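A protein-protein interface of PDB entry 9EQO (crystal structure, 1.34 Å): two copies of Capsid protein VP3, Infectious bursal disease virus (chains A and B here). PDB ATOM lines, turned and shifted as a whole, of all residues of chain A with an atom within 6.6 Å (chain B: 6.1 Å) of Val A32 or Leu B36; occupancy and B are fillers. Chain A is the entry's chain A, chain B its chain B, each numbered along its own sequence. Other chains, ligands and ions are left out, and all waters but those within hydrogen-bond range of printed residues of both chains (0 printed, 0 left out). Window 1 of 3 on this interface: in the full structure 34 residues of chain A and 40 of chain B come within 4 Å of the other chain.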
ATOM      1  N   GLN A  27      -8.961  -0.648 -24.921  1.00  0.00           N
ATOM      2  CA  GLN A  27      -8.950   0.750 -24.500  1.00  0.00           C
ATOM      3  C   GLN A  27      -7.694   1.072 -23.696  1.00  0.00           C
ATOM      4  O   GLN A  27      -7.073   2.124 -23.890  1.00  0.00           O
ATOM      5  CB  GLN A  27     -10.215   1.075 -23.693  1.00  0.00           C
ATOM      6  CG  GLN A  27     -10.421   2.573 -23.382  1.00  0.00           C
ATOM      7  CD  GLN A  27     -11.055   3.310 -24.556  1.00  0.00           C
ATOM      8  OE1 GLN A  27     -10.371   3.934 -25.354  1.00  0.00           O
ATOM      9  NE2 GLN A  27     -12.374   3.196 -24.682  1.00  0.00           N
ATOM     10  N   SER A  28      -7.295   0.169 -22.803  1.00  0.00           N
ATOM     11  CA  SER A  28      -6.058   0.377 -22.057  1.00  0.00           C
ATOM     12  C   SER A  28      -4.858   0.436 -22.988  1.00  0.00           C
ATOM     13  O   SER A  28      -3.978   1.292 -22.823  1.00  0.00           O
ATOM     14  CB  SER A  28      -5.887  -0.730 -21.020  1.00  0.00           C
ATOM     15  OG  SER A  28      -6.893  -0.637 -20.029  1.00  0.00           O
ATOM     16  N   ALA A  29      -4.813  -0.451 -23.982  1.00  0.00           N
ATOM     17  CA  ALA A  29      -3.715  -0.440 -24.940  1.00  0.00           C
ATOM     18  C   ALA A  29      -3.705   0.849 -25.753  1.00  0.00           C
ATOM     19  O   ALA A  29      -2.640   1.432 -25.987  1.00  0.00           O
ATOM     20  CB  ALA A  29      -3.806  -1.660 -25.850  1.00  0.00           C
ATOM     21  N   LEU A  30      -4.880   1.323 -26.167  1.00  0.00           N
ATOM     22  CA  LEU A  30      -4.958   2.576 -26.907  1.00  0.00           C
ATOM     23  C   LEU A  30      -4.487   3.743 -26.051  1.00  0.00           C
ATOM     24  O   LEU A  30      -3.782   4.637 -26.537  1.00  0.00           O
ATOM     25  CB  LEU A  30      -6.385   2.802 -27.408  1.00  0.00           C
ATOM     26  CG  LEU A  30      -6.639   4.127 -28.130  1.00  0.00           C
ATOM     27  CD1 LEU A  30      -5.725   4.289 -29.328  1.00  0.00           C
ATOM     28  CD2 LEU A  30      -8.099   4.194 -28.560  1.00  0.00           C
ATOM     29  N   SER A  31      -4.848   3.742 -24.763  1.00  0.00           N
ATOM     30  CA  SER A  31      -4.372   4.787 -23.861  1.00  0.00           C
ATOM     31  C   SER A  31      -2.853   4.771 -23.758  1.00  0.00           C
ATOM     32  O   SER A  31      -2.211   5.830 -23.749  1.00  0.00           O
ATOM     33  CB  SER A  31      -5.017   4.628 -22.482  1.00  0.00           C
ATOM     34  OG  SER A  31      -6.418   4.832 -22.586  1.00  0.00           O
ATOM     35  N   VAL A  32      -2.249   3.578 -23.698  1.00  0.00           N
ATOM     36  CA  VAL A  32      -0.791   3.486 -23.698  1.00  0.00           C
ATOM     37  C   VAL A  32      -0.224   4.037 -24.999  1.00  0.00           C
ATOM     38  O   VAL A  32       0.754   4.801 -24.995  1.00  0.00           O
ATOM     39  CB  VAL A  32      -0.338   2.035 -23.436  1.00  0.00           C
ATOM     40  CG1 VAL A  32       1.186   1.896 -23.658  1.00  0.00           C
ATOM     41  CG2 VAL A  32      -0.695   1.614 -22.021  1.00  0.00           C
ATOM     42  N   PHE A  33      -0.832   3.672 -26.131  1.00  0.00           N
ATOM     43  CA  PHE A  33      -0.370   4.171 -27.422  1.00  0.00           C
ATOM     44  C   PHE A  33      -0.398   5.693 -27.464  1.00  0.00           C
ATOM     45  O   PHE A  33       0.572   6.330 -27.889  1.00  0.00           O
ATOM     46  CB  PHE A  33      -1.201   3.587 -28.566  1.00  0.00           C
ATOM     47  CG  PHE A  33      -0.901   4.229 -29.888  1.00  0.00           C
ATOM     48  CD1 PHE A  33       0.306   3.984 -30.530  1.00  0.00           C
ATOM     49  CD2 PHE A  33      -1.786   5.135 -30.455  1.00  0.00           C
ATOM     50  CE1 PHE A  33       0.605   4.598 -31.736  1.00  0.00           C
ATOM     51  CE2 PHE A  33      -1.497   5.750 -31.668  1.00  0.00           C
ATOM     52  CZ  PHE A  33      -0.301   5.478 -32.306  1.00  0.00           C
ATOM     53  N   MET A  34      -1.506   6.298 -27.028  1.00  0.00           N
ATOM     54  CA  MET A  34      -1.615   7.751 -27.085  1.00  0.00           C
ATOM     55  C   MET A  34      -0.586   8.413 -26.185  1.00  0.00           C
ATOM     56  O   MET A  34      -0.033   9.463 -26.530  1.00  0.00           O
ATOM     57  CB  MET A  34      -3.022   8.199 -26.709  1.00  0.00           C
ATOM     58  CG  MET A  34      -4.078   7.732 -27.707  1.00  0.00           C
ATOM     59  SD  MET A  34      -5.725   8.294 -27.266  1.00  0.00           S
ATOM     60  CE  MET A  34      -5.905   7.650 -25.603  1.00  0.00           C
ATOM     61  N   TRP A  35      -0.317   7.814 -25.024  1.00  0.00           N
ATOM     62  CA  TRP A  35       0.684   8.347 -24.111  1.00  0.00           C
ATOM     63  C   TRP A  35       2.083   8.234 -24.699  1.00  0.00           C
ATOM     64  O   TRP A  35       2.869   9.191 -24.639  1.00  0.00           O
ATOM     65  CB  TRP A  35       0.564   7.582 -22.798  1.00  0.00           C
ATOM     66  CG  TRP A  35       1.639   7.795 -21.792  1.00  0.00           C
ATOM     67  CD1 TRP A  35       1.869   8.923 -21.049  1.00  0.00           C
ATOM     68  CD2 TRP A  35       2.602   6.826 -21.363  1.00  0.00           C
ATOM     69  NE1 TRP A  35       2.927   8.712 -20.195  1.00  0.00           N
ATOM     70  CE2 TRP A  35       3.391   7.432 -20.367  1.00  0.00           C
ATOM     71  CE3 TRP A  35       2.869   5.498 -21.722  1.00  0.00           C
ATOM     72  CZ2 TRP A  35       4.427   6.762 -19.731  1.00  0.00           C
ATOM     73  CZ3 TRP A  35       3.894   4.834 -21.088  1.00  0.00           C
ATOM     74  CH2 TRP A  35       4.663   5.465 -20.102  1.00  0.00           C
ATOM     75  N   LEU A  36       2.412   7.075 -25.276  1.00  0.00           N
ATOM     76  CA  LEU A  36       3.712   6.916 -25.920  1.00  0.00           C
ATOM     77  C   LEU A  36       3.862   7.863 -27.104  1.00  0.00           C
ATOM     78  O   LEU A  36       4.929   8.455 -27.309  1.00  0.00           O
ATOM     79  CB  LEU A  36       3.889   5.468 -26.374  1.00  0.00           C
ATOM     80  CG  LEU A  36       3.972   4.361 -25.320  1.00  0.00           C
ATOM     81  CD1 LEU A  36       3.950   3.017 -26.025  1.00  0.00           C
ATOM     82  CD2 LEU A  36       5.202   4.497 -24.457  1.00  0.00           C
ATOM     83  N   GLU A  37       2.795   8.046 -27.877  1.00  0.00           N
ATOM     84  CA  GLU A  37       2.881   8.885 -29.064  1.00  0.00           C
ATOM     85  C   GLU A  37       3.039  10.353 -28.688  1.00  0.00           C
ATOM     86  O   GLU A  37       3.884  11.055 -29.260  1.00  0.00           O
ATOM     87  CB  GLU A  37       1.647   8.673 -29.936  1.00  0.00           C
ATOM     88  CG  GLU A  37       1.800   9.222 -31.350  1.00  0.00           C
ATOM     89  CD  GLU A  37       1.595  10.720 -31.434  1.00  0.00           C
ATOM     90  OE1 GLU A  37       0.862  11.269 -30.583  1.00  0.00           O
ATOM     91  OE2 GLU A  37       2.178  11.348 -32.350  1.00  0.00           O
ATOM     92  N   VAL A  42       7.127   5.847 -28.887  1.00  0.00           N
ATOM     93  CA  VAL A  42       6.579   4.580 -29.386  1.00  0.00           C
ATOM     94  C   VAL A  42       7.691   3.676 -29.913  1.00  0.00           C
ATOM     95  O   VAL A  42       7.757   2.492 -29.573  1.00  0.00           O
ATOM     96  CB  VAL A  42       5.486   4.801 -30.449  1.00  0.00           C
ATOM     97  CG1 VAL A  42       4.894   3.449 -30.868  1.00  0.00           C
ATOM     98  CG2 VAL A  42       4.384   5.706 -29.919  1.00  0.00           C
ATOM     99  N   MET A  45       9.887   2.384 -27.189  1.00  0.00           N
ATOM    100  CA  MET A  45       9.293   1.255 -26.477  1.00  0.00           C
ATOM    101  C   MET A  45       9.414  -0.037 -27.280  1.00  0.00           C
ATOM    102  O   MET A  45       9.680  -1.104 -26.714  1.00  0.00           O
ATOM    103  CB  MET A  45       7.832   1.546 -26.127  1.00  0.00           C
ATOM    104  CG  MET A  45       7.191   0.476 -25.235  1.00  0.00           C
ATOM    105  SD  MET A  45       7.953   0.312 -23.610  1.00  0.00           S
ATOM    106  CE  MET A  45       7.358   1.809 -22.825  1.00  0.00           C
ATOM    107  N   MET A  58      10.743  -4.909 -17.552  1.00  0.00           N
ATOM    108  CA  MET A  58       9.625  -3.976 -17.510  1.00  0.00           C
ATOM    109  C   MET A  58       8.665  -4.296 -16.372  1.00  0.00           C
ATOM    110  O   MET A  58       8.187  -3.385 -15.690  1.00  0.00           O
ATOM    111  CB  MET A  58       8.906  -3.939 -18.856  1.00  0.00           C
ATOM    112  CG  MET A  58       7.754  -2.929 -18.891  1.00  0.00           C
ATOM    113  SD  MET A  58       8.251  -1.204 -18.586  1.00  0.00           S
ATOM    114  CE  MET A  58       8.953  -0.758 -20.169  1.00  0.00           C
ATOM    115  N   LEU A  62       7.446  -1.664 -13.545  1.00  0.00           N
ATOM    116  CA  LEU A  62       6.051  -1.299 -13.333  1.00  0.00           C
ATOM    117  C   LEU A  62       5.580  -1.678 -11.933  1.00  0.00           C
ATOM    118  O   LEU A  62       4.781  -0.952 -11.328  1.00  0.00           O
ATOM    119  CB  LEU A  62       5.171  -1.936 -14.410  1.00  0.00           C
ATOM    120  CG  LEU A  62       5.472  -1.556 -15.864  1.00  0.00           C
ATOM    121  CD1 LEU A  62       4.572  -2.335 -16.814  1.00  0.00           C
ATOM    122  CD2 LEU A  62       5.328  -0.053 -16.098  1.00  0.00           C
ATOM    123  N   SER B  31       4.077  -3.765 -32.828  1.00  0.00           N
ATOM    124  CA  SER B  31       5.002  -4.553 -32.021  1.00  0.00           C
ATOM    125  C   SER B  31       4.761  -4.336 -30.537  1.00  0.00           C
ATOM    126  O   SER B  31       4.777  -5.289 -29.749  1.00  0.00           O
ATOM    127  CB  SER B  31       6.435  -4.174 -32.377  1.00  0.00           C
ATOM    128  OG  SER B  31       6.713  -4.472 -33.736  1.00  0.00           O
ATOM    129  N   VAL B  32       4.517  -3.085 -30.131  1.00  0.00           N
ATOM    130  CA  VAL B  32       4.293  -2.794 -28.720  1.00  0.00           C
ATOM    131  C   VAL B  32       2.995  -3.424 -28.238  1.00  0.00           C
ATOM    132  O   VAL B  32       2.949  -4.005 -27.152  1.00  0.00           O
ATOM    133  CB  VAL B  32       4.336  -1.276 -28.476  1.00  0.00           C
ATOM    134  CG1 VAL B  32       3.846  -0.945 -27.073  1.00  0.00           C
ATOM    135  CG2 VAL B  32       5.764  -0.744 -28.666  1.00  0.00           C
ATOM    136  N   PHE B  33       1.924  -3.314 -29.031  1.00  0.00           N
ATOM    137  CA  PHE B  33       0.654  -3.936 -28.658  1.00  0.00           C
ATOM    138  C   PHE B  33       0.822  -5.438 -28.449  1.00  0.00           C
ATOM    139  O   PHE B  33       0.354  -5.988 -27.446  1.00  0.00           O
ATOM    140  CB  PHE B  33      -0.413  -3.657 -29.716  1.00  0.00           C
ATOM    141  CG  PHE B  33      -1.144  -2.362 -29.522  1.00  0.00           C
ATOM    142  CD1 PHE B  33      -0.485  -1.221 -29.118  1.00  0.00           C
ATOM    143  CD2 PHE B  33      -2.506  -2.287 -29.750  1.00  0.00           C
ATOM    144  CE1 PHE B  33      -1.172  -0.039 -28.940  1.00  0.00           C
ATOM    145  CE2 PHE B  33      -3.188  -1.103 -29.579  1.00  0.00           C
ATOM    146  CZ  PHE B  33      -2.514   0.021 -29.181  1.00  0.00           C
ATOM    147  N   MET B  34       1.511  -6.111 -29.375  1.00  0.00           N
ATOM    148  CA  MET B  34       1.700  -7.552 -29.250  1.00  0.00           C
ATOM    149  C   MET B  34       2.508  -7.889 -28.003  1.00  0.00           C
ATOM    150  O   MET B  34       2.176  -8.831 -27.274  1.00  0.00           O
ATOM    151  CB  MET B  34       2.385  -8.094 -30.499  1.00  0.00           C
ATOM    152  CG  MET B  34       1.536  -7.987 -31.751  1.00  0.00           C
ATOM    153  SD  MET B  34       2.320  -8.736 -33.198  1.00  0.00           S
ATOM    154  CE  MET B  34       3.764  -7.699 -33.412  1.00  0.00           C
ATOM    155  N   TRP B  35       3.549  -7.109 -27.727  1.00  0.00           N
ATOM    156  CA  TRP B  35       4.421  -7.374 -26.592  1.00  0.00           C
ATOM    157  C   TRP B  35       3.696  -7.142 -25.273  1.00  0.00           C
ATOM    158  O   TRP B  35       3.831  -7.938 -24.340  1.00  0.00           O
ATOM    159  CB  TRP B  35       5.649  -6.481 -26.723  1.00  0.00           C
ATOM    160  CG  TRP B  35       6.665  -6.519 -25.616  1.00  0.00           C
ATOM    161  CD1 TRP B  35       7.586  -7.501 -25.367  1.00  0.00           C
ATOM    162  CD2 TRP B  35       6.915  -5.484 -24.658  1.00  0.00           C
ATOM    163  NE1 TRP B  35       8.391  -7.140 -24.308  1.00  0.00           N
ATOM    164  CE2 TRP B  35       7.992  -5.910 -23.850  1.00  0.00           C
ATOM    165  CE3 TRP B  35       6.333  -4.240 -24.407  1.00  0.00           C
ATOM    166  CZ2 TRP B  35       8.510  -5.125 -22.810  1.00  0.00           C
ATOM    167  CZ3 TRP B  35       6.844  -3.459 -23.372  1.00  0.00           C
ATOM    168  CH2 TRP B  35       7.925  -3.909 -22.588  1.00  0.00           C
ATOM    169  N   LEU B  36       2.928  -6.055 -25.180  1.00  0.00           N
ATOM    170  CA  LEU B  36       2.152  -5.810 -23.966  1.00  0.00           C
ATOM    171  C   LEU B  36       1.127  -6.908 -23.733  1.00  0.00           C
ATOM    172  O   LEU B  36       0.937  -7.363 -22.602  1.00  0.00           O
ATOM    173  CB  LEU B  36       1.434  -4.471 -24.059  1.00  0.00           C
ATOM    174  CG  LEU B  36       2.273  -3.198 -24.094  1.00  0.00           C
ATOM    175  CD1 LEU B  36       1.343  -2.036 -24.354  1.00  0.00           C
ATOM    176  CD2 LEU B  36       3.045  -3.004 -22.792  1.00  0.00           C
ATOM    177  N   GLU B  37       0.424  -7.318 -24.790  1.00  0.00           N
ATOM    178  CA  GLU B  37      -0.611  -8.333 -24.641  1.00  0.00           C
ATOM    179  C   GLU B  37      -0.008  -9.678 -24.268  1.00  0.00           C
ATOM    180  O   GLU B  37      -0.493 -10.347 -23.350  1.00  0.00           O
ATOM    181  CB  GLU B  37      -1.426  -8.447 -25.929  1.00  0.00           C
ATOM    182  CG  GLU B  37      -2.583  -9.411 -25.796  1.00  0.00           C
ATOM    183  CD  GLU B  37      -3.220  -9.789 -27.119  1.00  0.00           C
ATOM    184  OE1 GLU B  37      -2.579  -9.601 -28.174  1.00  0.00           O
ATOM    185  OE2 GLU B  37      -4.374 -10.280 -27.094  1.00  0.00           O
ATOM    186  N   GLU B  38       1.048 -10.096 -24.970  1.00  0.00           N
ATOM    187  CA  GLU B  38       1.635 -11.403 -24.703  1.00  0.00           C
ATOM    188  C   GLU B  38       2.190 -11.484 -23.291  1.00  0.00           C
ATOM    189  O   GLU B  38       2.125 -12.535 -22.651  1.00  0.00           O
ATOM    190  CB  GLU B  38       2.740 -11.704 -25.709  1.00  0.00           C
ATOM    191  CG  GLU B  38       2.252 -11.986 -27.111  1.00  0.00           C
ATOM    192  CD  GLU B  38       3.392 -12.104 -28.104  1.00  0.00           C
ATOM    193  OE1 GLU B  38       4.562 -11.925 -27.695  1.00  0.00           O
ATOM    194  OE2 GLU B  38       3.120 -12.372 -29.295  1.00  0.00           O
ATOM    195  N   ASN B  39       2.738 -10.384 -22.787  1.00  0.00           N
ATOM    196  CA  ASN B  39       3.349 -10.383 -21.469  1.00  0.00           C
ATOM    197  C   ASN B  39       2.385 -10.002 -20.355  1.00  0.00           C
ATOM    198  O   ASN B  39       2.782  -9.989 -19.187  1.00  0.00           O
ATOM    199  CB  ASN B  39       4.600  -9.502 -21.491  1.00  0.00           C
ATOM    200  CG  ASN B  39       5.719 -10.148 -22.265  1.00  0.00           C
ATOM    201  OD1 ASN B  39       6.140 -11.258 -21.943  1.00  0.00           O
ATOM    202  ND2 ASN B  39       6.177  -9.491 -23.316  1.00  0.00           N
ATOM    203  N   GLY B  40       1.124  -9.737 -20.680  1.00  0.00           N
ATOM    204  CA  GLY B  40       0.137  -9.462 -19.659  1.00  0.00           C
ATOM    205  C   GLY B  40       0.337  -8.155 -18.928  1.00  0.00           C
ATOM    206  O   GLY B  40      -0.028  -8.051 -17.757  1.00  0.00           O
ATOM    207  N   ILE B  41       0.914  -7.149 -19.588  1.00  0.00           N
ATOM    208  CA  ILE B  41       1.220  -5.876 -18.947  1.00  0.00           C
ATOM    209  C   ILE B  41       0.485  -4.695 -19.589  1.00  0.00           C
ATOM    210  O   ILE B  41       0.888  -3.555 -19.400  1.00  0.00           O
ATOM    211  CB  ILE B  41       2.739  -5.631 -18.826  1.00  0.00           C
ATOM    212  CG1 ILE B  41       3.416  -5.680 -20.199  1.00  0.00           C
ATOM    213  CG2 ILE B  41       3.355  -6.632 -17.865  1.00  0.00           C
ATOM    214  CD1 ILE B  41       4.827  -5.082 -20.209  1.00  0.00           C
ATOM    215  N   VAL B  42      -0.605  -4.937 -20.328  1.00  0.00           N
ATOM    216  CA  VAL B  42      -1.365  -3.830 -20.911  1.00  0.00           C
ATOM    217  C   VAL B  42      -1.910  -2.925 -19.815  1.00  0.00           C
ATOM    218  O   VAL B  42      -1.708  -1.706 -19.825  1.00  0.00           O
ATOM    219  CB  VAL B  42      -2.510  -4.345 -21.800  1.00  0.00           C
ATOM    220  CG1 VAL B  42      -3.331  -3.165 -22.312  1.00  0.00           C
ATOM    221  CG2 VAL B  42      -1.986  -5.188 -22.959  1.00  0.00           C
ATOM    222  N   MET B  45       0.827  -1.179 -17.739  1.00  0.00           N
ATOM    223  CA  MET B  45       1.426  -0.024 -18.390  1.00  0.00           C
ATOM    224  C   MET B  45       0.459   1.148 -18.456  1.00  0.00           C
ATOM    225  O   MET B  45       0.865   2.300 -18.297  1.00  0.00           O
ATOM    226  CB  MET B  45       1.929  -0.397 -19.775  1.00  0.00           C
ATOM    227  CG  MET B  45       2.596   0.794 -20.446  1.00  0.00           C
ATOM    228  SD  MET B  45       4.014   0.586 -21.563  1.00  0.00           S
ATOM    229  CE  MET B  45       5.094  -0.519 -20.645  1.00  0.00           C
ATOM    230  N   ALA B  46      -0.826   0.880 -18.691  1.00  0.00           N
ATOM    231  CA  ALA B  46      -1.808   1.960 -18.679  1.00  0.00           C
ATOM    232  C   ALA B  46      -1.864   2.630 -17.312  1.00  0.00           C
ATOM    233  O   ALA B  46      -1.937   3.861 -17.211  1.00  0.00           O
ATOM    234  CB  ALA B  46      -3.183   1.425 -19.078  1.00  0.00           C
ATOM    235  N   ASN B  47      -1.792   1.830 -16.249  1.00  0.00           N
ATOM    236  CA  ASN B  47      -1.773   2.391 -14.904  1.00  0.00           C
ATOM    237  C   ASN B  47      -0.517   3.222 -14.670  1.00  0.00           C
ATOM    238  O   ASN B  47      -0.579   4.307 -14.082  1.00  0.00           O
ATOM    239  CB  ASN B  47      -1.866   1.261 -13.884  1.00  0.00           C
ATOM    240  CG  ASN B  47      -1.837   1.765 -12.471  1.00  0.00           C
ATOM    241  OD1 ASN B  47      -2.719   2.511 -12.058  1.00  0.00           O
ATOM    242  ND2 ASN B  47      -0.812   1.376 -11.722  1.00  0.00           N
ATOM    243  N   ALA B  49       1.180   4.850 -16.915  1.00  0.00           N
ATOM    244  CA  ALA B  49       1.083   6.069 -17.708  1.00  0.00           C
ATOM    245  C   ALA B  49       0.298   7.149 -16.986  1.00  0.00           C
ATOM    246  O   ALA B  49       0.625   8.336 -17.113  1.00  0.00           O
ATOM    247  CB  ALA B  49       0.457   5.761 -19.071  1.00  0.00           C
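Val A32 touches Met B45, and with the chains exchanged Met A45 touches Val B32. Phe B33 touches its own counterpart, Phe A33. Val A42 touches Val B32, but with the chains exchanged Val A32 does not touch Val B42 (4.1 Å). Met A45 touches Trp B35, but with the chains exchanged Trp A35 does not touch Met B45 (4.3 Å).
Printed residues of chain B within 4 Å of Val A32: Leu B36 (3.996 Å), Met B45 (3.7 Å) and Ala B46 (3.4 Å). Of the printed residues of chain A, Leu B36 touches Val A32. Printed residues of chain A within 4 Å of Trp B35: Met A45 (3.9 Å) and Met A58 (3.8 Å). Of the printed residues of chain B, Met A45 touches Val B32, Trp B35 and Met B45. Of the printed residues of chain B, Trp A35 touches Ala B49 (3.3 Å). Of the printed residues of chain B, Ala A29 touches Phe B33 and Val B42. Of the printed residues of chain A, Ala B49 touches Trp A35 (3.3 Å). Leu A36 touches none of the printed residues of chain B. The nearest printed residue of chain A that does not touch Leu B36 is Ala A29 (5.3 Å). The nearest printed residue of chain A that does not touch Ile B41 is Leu A62 (4.3 Å).
Of the 15 printed residues of chain A, 8 touch a printed residue of chain B. Of the 16 printed residues of chain B, 9 touch a printed residue of chain A. Printed residues of chain B that touch a printed residue of chain A: Val B32, Phe B33, Trp B35, Leu B36, Ile B41, Val B42, Met B45, Ala B46 and Ala B49. Among the printed residues, 16 pairs touch across the chains.
N of Ile B41 is in hydrogen-bond range of O of Leu B36 (3.0 Å). O of Trp B35 sits at hydrogen-bond distance from ND2 of Asn B39 (3.0 Å).
Among the printed residues, pairs that only touch across the chains: Ser A28 with Val B42 (3.8 Å), Ser A28 with Ala B46 (3.8 Å), Ala A29 with Phe B33 (3.5 Å), Ala A29 with Val B42 (3.5 Å), Val A32 with Leu B36 (3.996 Å), Val A32 with Met B45 (3.7 Å), Val A32 with Ala B46 (3.4 Å), Phe A33 with Phe B33 (3.6 Å), Trp A35 with Ala B49 (3.3 Å), Val A42 with Val B32 (3.9 Å), Met A45 with Val B32 (3.9 Å), Met A45 with Trp B35 (3.9 Å), Met A45 with Met B45 (3.8 Å), Met A58 with Trp B35 (3.8 Å), Met A58 with Ile B41 (3.9 Å) and Met A58 with Met B45 (3.8 Å).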
